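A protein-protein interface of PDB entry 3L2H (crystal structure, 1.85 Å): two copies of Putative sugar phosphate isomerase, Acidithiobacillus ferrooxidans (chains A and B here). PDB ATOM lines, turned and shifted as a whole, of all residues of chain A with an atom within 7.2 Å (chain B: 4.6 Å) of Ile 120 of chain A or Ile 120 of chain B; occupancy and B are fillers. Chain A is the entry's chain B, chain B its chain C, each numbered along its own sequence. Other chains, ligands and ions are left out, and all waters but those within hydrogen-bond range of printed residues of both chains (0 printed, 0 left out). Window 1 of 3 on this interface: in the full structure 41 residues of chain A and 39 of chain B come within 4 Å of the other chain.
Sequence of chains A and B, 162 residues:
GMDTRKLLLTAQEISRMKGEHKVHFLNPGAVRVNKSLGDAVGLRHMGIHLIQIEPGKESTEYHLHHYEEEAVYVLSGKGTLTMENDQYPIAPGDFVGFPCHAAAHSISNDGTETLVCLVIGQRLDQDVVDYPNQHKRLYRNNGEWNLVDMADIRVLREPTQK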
ATOM      1  N   LEU A  43     -34.813  29.400  14.844  1.00  0.00           N
ATOM      2  CA  LEU A  43     -35.361  28.991  16.151  1.00  0.00           C
ATOM      3  C   LEU A  43     -36.071  30.141  16.852  1.00  0.00           C
ATOM      4  O   LEU A  43     -35.601  31.295  16.842  1.00  0.00           O
ATOM      5  CB  LEU A  43     -34.289  28.426  17.065  1.00  0.00           C
ATOM      6  CG  LEU A  43     -33.508  27.236  16.521  1.00  0.00           C
ATOM      7  CD1 LEU A  43     -32.432  26.872  17.542  1.00  0.00           C
ATOM      8  CD2 LEU A  43     -34.397  26.050  16.227  1.00  0.00           C
ATOM      9  N   MET A  46     -35.972  29.058  21.810  1.00  0.00           N
ATOM     10  CA  MET A  46     -34.681  28.960  22.463  1.00  0.00           C
ATOM     11  C   MET A  46     -33.773  29.939  21.756  1.00  0.00           C
ATOM     12  O   MET A  46     -33.970  30.233  20.571  1.00  0.00           O
ATOM     13  CB  MET A  46     -34.038  27.593  22.320  1.00  0.00           C
ATOM     14  CG  MET A  46     -34.953  26.404  22.395  1.00  0.00           C
ATOM     15  SD  MET A  46     -33.874  24.729  22.301  1.00  0.00           S
ATOM     16  CE  MET A  46     -33.057  24.912  20.641  1.00  0.00           C
ATOM     17  N   GLY A  47     -32.788  30.409  22.496  1.00  0.00           N
ATOM     18  CA  GLY A  47     -31.738  31.292  22.032  1.00  0.00           C
ATOM     19  C   GLY A  47     -30.450  30.485  22.152  1.00  0.00           C
ATOM     20  O   GLY A  47     -30.185  29.831  23.187  1.00  0.00           O
ATOM     21  N   ILE A  48     -29.702  30.396  21.069  1.00  0.00           N
ATOM     22  CA  ILE A  48     -28.409  29.773  21.083  1.00  0.00           C
ATOM     23  C   ILE A  48     -27.440  30.784  20.451  1.00  0.00           C
ATOM     24  O   ILE A  48     -27.586  31.111  19.267  1.00  0.00           O
ATOM     25  CB  ILE A  48     -28.383  28.443  20.338  1.00  0.00           C
ATOM     26  CG1 ILE A  48     -29.394  27.458  20.940  1.00  0.00           C
ATOM     27  CG2 ILE A  48     -26.923  27.834  20.383  1.00  0.00           C
ATOM     28  CD1 ILE A  48     -29.605  26.119  20.227  1.00  0.00           C
ATOM     29  N   HIS A  49     -26.463  31.218  21.244  1.00  0.00           N
ATOM     30  CA  HIS A  49     -25.579  32.316  20.921  1.00  0.00           C
ATOM     31  C   HIS A  49     -24.121  31.886  21.113  1.00  0.00           C
ATOM     32  O   HIS A  49     -23.755  31.334  22.156  1.00  0.00           O
ATOM     33  CB  HIS A  49     -25.873  33.512  21.834  1.00  0.00           C
ATOM     34  CG  HIS A  49     -27.277  34.017  21.751  1.00  0.00           C
ATOM     35  ND1 HIS A  49     -27.681  34.933  20.794  1.00  0.00           N
ATOM     36  CD2 HIS A  49     -28.384  33.722  22.482  1.00  0.00           C
ATOM     37  CE1 HIS A  49     -28.963  35.211  20.976  1.00  0.00           C
ATOM     38  NE2 HIS A  49     -29.412  34.490  21.992  1.00  0.00           N
ATOM     39  N   GLU A  69     -34.845  29.463  31.921  1.00  0.00           N
ATOM     40  CA  GLU A  69     -33.570  28.811  32.172  1.00  0.00           C
ATOM     41  C   GLU A  69     -32.479  29.363  31.250  1.00  0.00           C
ATOM     42  O   GLU A  69     -32.753  29.857  30.159  1.00  0.00           O
ATOM     43  CB  GLU A  69     -33.714  27.279  31.989  1.00  0.00           C
ATOM     44  CG  GLU A  69     -34.566  26.715  33.129  1.00  0.00           C
ATOM     45  CD  GLU A  69     -34.698  25.224  33.100  1.00  0.00           C
ATOM     46  OE1 GLU A  69     -34.480  24.653  32.023  1.00  0.00           O
ATOM     47  OE2 GLU A  69     -35.043  24.652  34.162  1.00  0.00           O
ATOM     48  N   GLU A  70     -31.227  29.256  31.691  1.00  0.00           N
ATOM     49  CA  GLU A  70     -30.093  29.770  30.947  1.00  0.00           C
ATOM     50  C   GLU A  70     -28.927  28.819  31.228  1.00  0.00           C
ATOM     51  O   GLU A  70     -28.875  28.251  32.316  1.00  0.00           O
ATOM     52  CB  GLU A  70     -29.774  31.184  31.464  1.00  0.00           C
ATOM     53  CG  GLU A  70     -28.673  31.871  30.843  1.00  0.00           C
ATOM     54  CD  GLU A  70     -28.631  33.359  31.217  1.00  0.00           C
ATOM     55  OE1 GLU A  70     -28.961  33.782  32.372  1.00  0.00           O
ATOM     56  OE2 GLU A  70     -28.272  34.091  30.305  1.00  0.00           O
ATOM     57  N   ALA A  71     -27.989  28.694  30.295  1.00  0.00           N
ATOM     58  CA  ALA A  71     -26.784  27.909  30.513  1.00  0.00           C
ATOM     59  C   ALA A  71     -25.640  28.431  29.659  1.00  0.00           C
ATOM     60  O   ALA A  71     -25.871  29.113  28.652  1.00  0.00           O
ATOM     61  CB  ALA A  71     -27.038  26.421  30.208  1.00  0.00           C
ATOM     62  N   VAL A  72     -24.406  28.088  30.050  1.00  0.00           N
ATOM     63  CA  VAL A  72     -23.198  28.542  29.364  1.00  0.00           C
ATOM     64  C   VAL A  72     -22.256  27.378  29.173  1.00  0.00           C
ATOM     65  O   VAL A  72     -22.057  26.590  30.097  1.00  0.00           O
ATOM     66  CB  VAL A  72     -22.469  29.660  30.126  1.00  0.00           C
ATOM     67  CG1 VAL A  72     -21.202  30.114  29.343  1.00  0.00           C
ATOM     68  CG2 VAL A  72     -23.395  30.866  30.417  1.00  0.00           C
ATOM     69  N   TYR A  73     -21.690  27.221  27.973  1.00  0.00           N
ATOM     70  CA  TYR A  73     -20.683  26.175  27.716  1.00  0.00           C
ATOM     71  C   TYR A  73     -19.440  26.856  27.167  1.00  0.00           C
ATOM     72  O   TYR A  73     -19.506  27.600  26.185  1.00  0.00           O
ATOM     73  CB  TYR A  73     -21.206  25.063  26.785  1.00  0.00           C
ATOM     74  CG  TYR A  73     -20.234  23.901  26.583  1.00  0.00           C
ATOM     75  CD1 TYR A  73     -20.229  22.838  27.461  1.00  0.00           C
ATOM     76  CD2 TYR A  73     -19.334  23.869  25.529  1.00  0.00           C
ATOM     77  CE1 TYR A  73     -19.356  21.763  27.315  1.00  0.00           C
ATOM     78  CE2 TYR A  73     -18.436  22.786  25.382  1.00  0.00           C
ATOM     79  CZ  TYR A  73     -18.461  21.738  26.283  1.00  0.00           C
ATOM     80  OH  TYR A  73     -17.644  20.630  26.173  1.00  0.00           O
ATOM     81  N   PHE A  95     -19.300  23.791  32.038  1.00  0.00           N
ATOM     82  CA  PHE A  95     -20.679  24.039  31.796  1.00  0.00           C
ATOM     83  C   PHE A  95     -21.303  24.560  33.057  1.00  0.00           C
ATOM     84  O   PHE A  95     -21.084  23.987  34.143  1.00  0.00           O
ATOM     85  CB  PHE A  95     -21.356  22.727  31.424  1.00  0.00           C
ATOM     86  CG  PHE A  95     -22.870  22.831  31.261  1.00  0.00           C
ATOM     87  CD1 PHE A  95     -23.431  23.288  30.091  1.00  0.00           C
ATOM     88  CD2 PHE A  95     -23.717  22.504  32.318  1.00  0.00           C
ATOM     89  CE1 PHE A  95     -24.834  23.387  29.969  1.00  0.00           C
ATOM     90  CE2 PHE A  95     -25.081  22.579  32.186  1.00  0.00           C
ATOM     91  CZ  PHE A  95     -25.637  23.026  31.008  1.00  0.00           C
ATOM     92  N   VAL A  96     -22.121  25.600  32.918  1.00  0.00           N
ATOM     93  CA  VAL A  96     -22.895  26.096  34.031  1.00  0.00           C
ATOM     94  C   VAL A  96     -24.337  26.281  33.575  1.00  0.00           C
ATOM     95  O   VAL A  96     -24.595  26.775  32.458  1.00  0.00           O
ATOM     96  CB  VAL A  96     -22.236  27.384  34.658  1.00  0.00           C
ATOM     97  CG1 VAL A  96     -22.074  28.431  33.684  1.00  0.00           C
ATOM     98  CG2 VAL A  96     -23.052  27.923  35.852  1.00  0.00           C
ATOM     99  N   LEU A 118     -20.753  29.279  24.259  1.00  0.00           N
ATOM    100  CA  LEU A 118     -22.100  29.093  23.796  1.00  0.00           C
ATOM    101  C   LEU A 118     -23.013  29.460  24.951  1.00  0.00           C
ATOM    102  O   LEU A 118     -22.806  28.992  26.082  1.00  0.00           O
ATOM    103  CB  LEU A 118     -22.376  27.647  23.418  1.00  0.00           C
ATOM    104  CG  LEU A 118     -21.997  27.141  22.068  1.00  0.00           C
ATOM    105  CD1 LEU A 118     -22.442  25.669  22.015  1.00  0.00           C
ATOM    106  CD2 LEU A 118     -22.659  28.037  20.968  1.00  0.00           C
ATOM    107  N   VAL A 119     -23.952  30.358  24.700  1.00  0.00           N
ATOM    108  CA  VAL A 119     -24.980  30.706  25.645  1.00  0.00           C
ATOM    109  C   VAL A 119     -26.326  30.157  25.112  1.00  0.00           C
ATOM    110  O   VAL A 119     -26.720  30.423  23.961  1.00  0.00           O
ATOM    111  CB  VAL A 119     -25.029  32.220  25.912  1.00  0.00           C
ATOM    112  CG1 VAL A 119     -26.195  32.527  26.852  1.00  0.00           C
ATOM    113  CG2 VAL A 119     -23.699  32.695  26.513  1.00  0.00           C
ATOM    114  N   ILE A 120     -27.012  29.389  25.969  1.00  0.00           N
ATOM    115  CA  ILE A 120     -28.230  28.667  25.635  1.00  0.00           C
ATOM    116  C   ILE A 120     -29.300  29.102  26.598  1.00  0.00           C
ATOM    117  O   ILE A 120     -29.095  29.032  27.832  1.00  0.00           O
ATOM    118  CB  ILE A 120     -28.041  27.162  25.754  1.00  0.00           C
ATOM    119  CG1 ILE A 120     -26.946  26.662  24.804  1.00  0.00           C
ATOM    120  CG2 ILE A 120     -29.379  26.420  25.453  1.00  0.00           C
ATOM    121  CD1 ILE A 120     -26.215  25.423  25.284  1.00  0.00           C
ATOM    122  N   GLY A 121     -30.431  29.594  26.083  1.00  0.00           N
ATOM    123  CA  GLY A 121     -31.493  30.042  26.954  1.00  0.00           C
ATOM    124  C   GLY A 121     -32.888  29.860  26.393  1.00  0.00           C
ATOM    125  O   GLY A 121     -33.086  29.666  25.174  1.00  0.00           O
ATOM    126  N   GLN A 122     -33.855  29.803  27.286  1.00  0.00           N
ATOM    127  CA  GLN A 122     -35.247  29.702  26.849  1.00  0.00           C
ATOM    128  C   GLN A 122     -35.652  31.037  26.383  1.00  0.00           C
ATOM    129  O   GLN A 122     -35.093  32.046  26.856  1.00  0.00           O
ATOM    130  CB  GLN A 122     -36.190  29.343  27.973  1.00  0.00           C
ATOM    131  CG  GLN A 122     -36.085  27.999  28.515  1.00  0.00           C
ATOM    132  CD  GLN A 122     -37.164  27.758  29.518  1.00  0.00           C
ATOM    133  OE1 GLN A 122     -36.941  27.909  30.720  1.00  0.00           O
ATOM    134  NE2 GLN A 122     -38.367  27.424  29.039  1.00  0.00           N
ATOM    135  N   MET B  46     -35.014  22.660  29.468  1.00  0.00           N
ATOM    136  CA  MET B  46     -34.217  22.439  28.289  1.00  0.00           C
ATOM    137  C   MET B  46     -33.458  21.162  28.523  1.00  0.00           C
ATOM    138  O   MET B  46     -33.099  20.848  29.657  1.00  0.00           O
ATOM    139  CB  MET B  46     -33.222  23.565  28.119  1.00  0.00           C
ATOM    140  CG  MET B  46     -33.787  24.954  28.234  1.00  0.00           C
ATOM    141  SD  MET B  46     -32.366  26.322  28.010  1.00  0.00           S
ATOM    142  CE  MET B  46     -31.015  25.691  29.192  1.00  0.00           C
ATOM    143  N   GLY B  47     -33.237  20.432  27.447  1.00  0.00           N
ATOM    144  CA  GLY B  47     -32.302  19.301  27.462  1.00  0.00           C
ATOM    145  C   GLY B  47     -30.968  19.783  26.887  1.00  0.00           C
ATOM    146  O   GLY B  47     -30.953  20.372  25.800  1.00  0.00           O
ATOM    147  N   ILE B  48     -29.856  19.558  27.589  1.00  0.00           N
ATOM    148  CA  ILE B  48     -28.547  19.874  27.049  1.00  0.00           C
ATOM    149  C   ILE B  48     -27.711  18.627  27.312  1.00  0.00           C
ATOM    150  O   ILE B  48     -27.450  18.287  28.480  1.00  0.00           O
ATOM    151  CB  ILE B  48     -27.922  21.139  27.664  1.00  0.00           C
ATOM    152  CG1 ILE B  48     -28.785  22.358  27.363  1.00  0.00           C
ATOM    153  CG2 ILE B  48     -26.502  21.357  27.112  1.00  0.00           C
ATOM    154  CD1 ILE B  48     -28.375  23.597  28.161  1.00  0.00           C
ATOM    155  N   GLU B  69     -38.358  22.346  19.532  1.00  0.00           N
ATOM    156  CA  GLU B  69     -37.154  22.697  18.782  1.00  0.00           C
ATOM    157  C   GLU B  69     -35.975  21.860  19.263  1.00  0.00           C
ATOM    158  O   GLU B  69     -35.957  21.390  20.412  1.00  0.00           O
ATOM    159  CB  GLU B  69     -36.855  24.176  18.950  1.00  0.00           C
ATOM    160  CG  GLU B  69     -37.895  24.991  18.267  1.00  0.00           C
ATOM    161  CD  GLU B  69     -37.642  26.490  18.290  1.00  0.00           C
ATOM    162  OE1 GLU B  69     -36.965  26.981  19.200  1.00  0.00           O
ATOM    163  OE2 GLU B  69     -38.175  27.174  17.390  1.00  0.00           O
ATOM    164  N   GLU B  70     -34.990  21.666  18.370  1.00  0.00           N
ATOM    165  CA  GLU B  70     -33.837  20.873  18.647  1.00  0.00           C
ATOM    166  C   GLU B  70     -32.677  21.516  17.893  1.00  0.00           C
ATOM    167  O   GLU B  70     -32.908  22.127  16.854  1.00  0.00           O
ATOM    168  CB  GLU B  70     -34.135  19.497  18.015  1.00  0.00           C
ATOM    169  CG  GLU B  70     -33.267  18.439  18.348  1.00  0.00           C
ATOM    170  CD  GLU B  70     -33.591  17.119  17.633  1.00  0.00           C
ATOM    171  OE1 GLU B  70     -34.396  16.941  16.653  1.00  0.00           O
ATOM    172  OE2 GLU B  70     -32.995  16.223  18.159  1.00  0.00           O
ATOM    173  N   ALA B  71     -31.437  21.289  18.346  1.00  0.00           N
ATOM    174  CA  ALA B  71     -30.232  21.789  17.671  1.00  0.00           C
ATOM    175  C   ALA B  71     -29.070  20.929  18.044  1.00  0.00           C
ATOM    176  O   ALA B  71     -29.086  20.276  19.132  1.00  0.00           O
ATOM    177  CB  ALA B  71     -29.958  23.260  18.030  1.00  0.00           C
ATOM    178  N   LEU B 118     -22.913  18.499  21.230  1.00  0.00           N
ATOM    179  CA  LEU B 118     -23.901  18.969  22.148  1.00  0.00           C
ATOM    180  C   LEU B 118     -25.239  18.923  21.429  1.00  0.00           C
ATOM    181  O   LEU B 118     -25.365  19.433  20.287  1.00  0.00           O
ATOM    182  CB  LEU B 118     -23.632  20.394  22.563  1.00  0.00           C
ATOM    183  CG  LEU B 118     -22.578  20.723  23.565  1.00  0.00           C
ATOM    184  CD1 LEU B 118     -22.404  22.290  23.661  1.00  0.00           C
ATOM    185  CD2 LEU B 118     -22.939  20.061  24.920  1.00  0.00           C
ATOM    186  N   VAL B 119     -26.250  18.321  22.076  1.00  0.00           N
ATOM    187  CA  VAL B 119     -27.600  18.286  21.557  1.00  0.00           C
ATOM    188  C   VAL B 119     -28.429  19.114  22.524  1.00  0.00           C
ATOM    189  O   VAL B 119     -28.379  18.886  23.743  1.00  0.00           O
ATOM    190  CB  VAL B 119     -28.134  16.855  21.367  1.00  0.00           C
ATOM    191  CG1 VAL B 119     -29.624  16.915  20.951  1.00  0.00           C
ATOM    192  CG2 VAL B 119     -27.325  16.143  20.340  1.00  0.00           C
ATOM    193  N   ILE B 120     -29.154  20.096  21.979  1.00  0.00           N
ATOM    194  CA  ILE B 120     -29.858  21.109  22.736  1.00  0.00           C
ATOM    195  C   ILE B 120     -31.303  21.068  22.322  1.00  0.00           C
ATOM    196  O   ILE B 120     -31.642  21.117  21.116  1.00  0.00           O
ATOM    197  CB  ILE B 120     -29.291  22.509  22.469  1.00  0.00           C
ATOM    198  CG1 ILE B 120     -27.810  22.534  22.867  1.00  0.00           C
ATOM    199  CG2 ILE B 120     -30.071  23.578  23.238  1.00  0.00           C
ATOM    200  CD1 ILE B 120     -26.890  23.533  22.123  1.00  0.00           C
ATOM    201  N   GLY B 121     -32.181  20.943  23.299  1.00  0.00           N
ATOM    202  CA  GLY B 121     -33.591  20.778  22.966  1.00  0.00           C
ATOM    203  C   GLY B 121     -34.535  21.341  24.021  1.00  0.00           C
ATOM    204  O   GLY B 121     -34.172  21.568  25.178  1.00  0.00           O
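Of the printed residues of chain B, Ile 120 of chain A touches Met 46 and Ile 120.
Of the printed residues of chain A, Ile 120 of chain B touches Ile 48 (3.97 Å) and Ile 120 (3.7 Å).
Of the printed residues of chain B, Leu 43 of chain A touches Glu 69.
Printed residues of chain A within 4 Å of Ala 71 of chain B: Ile 48 (3.6 Å).
Printed residues of chain B within 4 Å of Tyr 73 of chain A: Leu 118.
Printed residues of chain B within 4 Å of Ile 48 of chain A: Ala 71 (3.6 Å) and Ile 120 (3.97 Å).
His 49 of chain A touches none of the printed residues of chain B.
The nearest printed residue of chain A that does not touch Ile 120 of chain B is Met 46 of chain A (4.1 Å).
The side-chain amide oxygen (OE1) of Gln 122 of chain A lies within hydrogen-bond range of the backbone NH (N) of Glu 69 of chain A (2.9 Å).
The backbone NH of Ala 71 of chain B sits at hydrogen-bond distance from the backbone carbonyl oxygen of Ile 120 of chain B (2.8 Å).
The backbone NH of Ala 71 of chain A sits at hydrogen-bond distance from the backbone carbonyl oxygen of Ile 120 of chain A (2.7 Å).
O of Leu 118 of chain A sits at hydrogen-bond distance from N of Tyr 73 of chain A (2.8 Å).
N of Gly 47 of chain A is in hydrogen-bond range of O of Gly 121 of chain A, 2.8 Å away.
The backbone carbonyl oxygen of Gly 121 of chain B sits at hydrogen-bond distance from the backbone NH of Gly 47 of chain B (2.7 Å).
Ile 48 of chain A touches Ala 71 of chain B, and with the chains exchanged Ala 71 of chain A touches Ile 48 of chain B.
Ile 48 of chain A touches Ile 120 of chain B, but with the chains exchanged Ile 120 of chain A does not touch Ile 48 of chain B (4.03 Å).
Leu 118 of chain B touches its own counterpart, Leu 118 of chain A.
Ile 120 of chain A touches its own counterpart, Ile 120 of chain B.
Positions printed for both chains: 46, 47, 48, 69, 70, 71, 118, 119, 120 and 121.
OE1 of Glu 69 of chain A lies within hydrogen-bond range of N of Met 46 of chain B (3.3 Å).
The backbone NH (N) of Met 46 of chain A sits at hydrogen-bond distance from the side-chain carboxylate (OE1) of Glu 69 of chain B (3.5 Å).
Of the 10 printed residues of chain B, 7 touch a printed residue of chain A.
Of the 17 printed residues of chain A, 11 touch a printed residue of chain B.
Among the printed residues, 14 pairs touch across the chains.
Among the printed residues, no Asp or Glu carboxylate lies within 4 Å of a Lys or Arg side-chain nitrogen of the other chain.
Leu 43 of chain A touches Glu 69 of chain B (CA to OE2, 3.6 Å).
Met 46 of chain A touches Gly 121 of chain B (SD to C, 3.9 Å).
Ile 48 of chain A touches Ala 71 of chain B (CD1 to CB, 3.6 Å).
CD2 of Tyr 73 of chain A touches CD1 of Leu 118 of chain B (3.9 Å).
Ile 48 of chain B touches Phe 95 of chain A.
Leu 118 of chain A touches Leu 118 of chain B (CD1 to CD1, 3.8 Å).
Ile 120 of chain A touches Met 46 of chain B (CG2 to SD, 3.9 Å).
Ile 120 of chain B touches Ile 120 of chain A (CG2 to CG2, 3.7 Å).
SD of Met 46 of chain B touches C of Gly 121 of chain A (3.9 Å).
CG of Met 46 of chain B touches CG of Gln 122 of chain A, 3.8 Å away.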
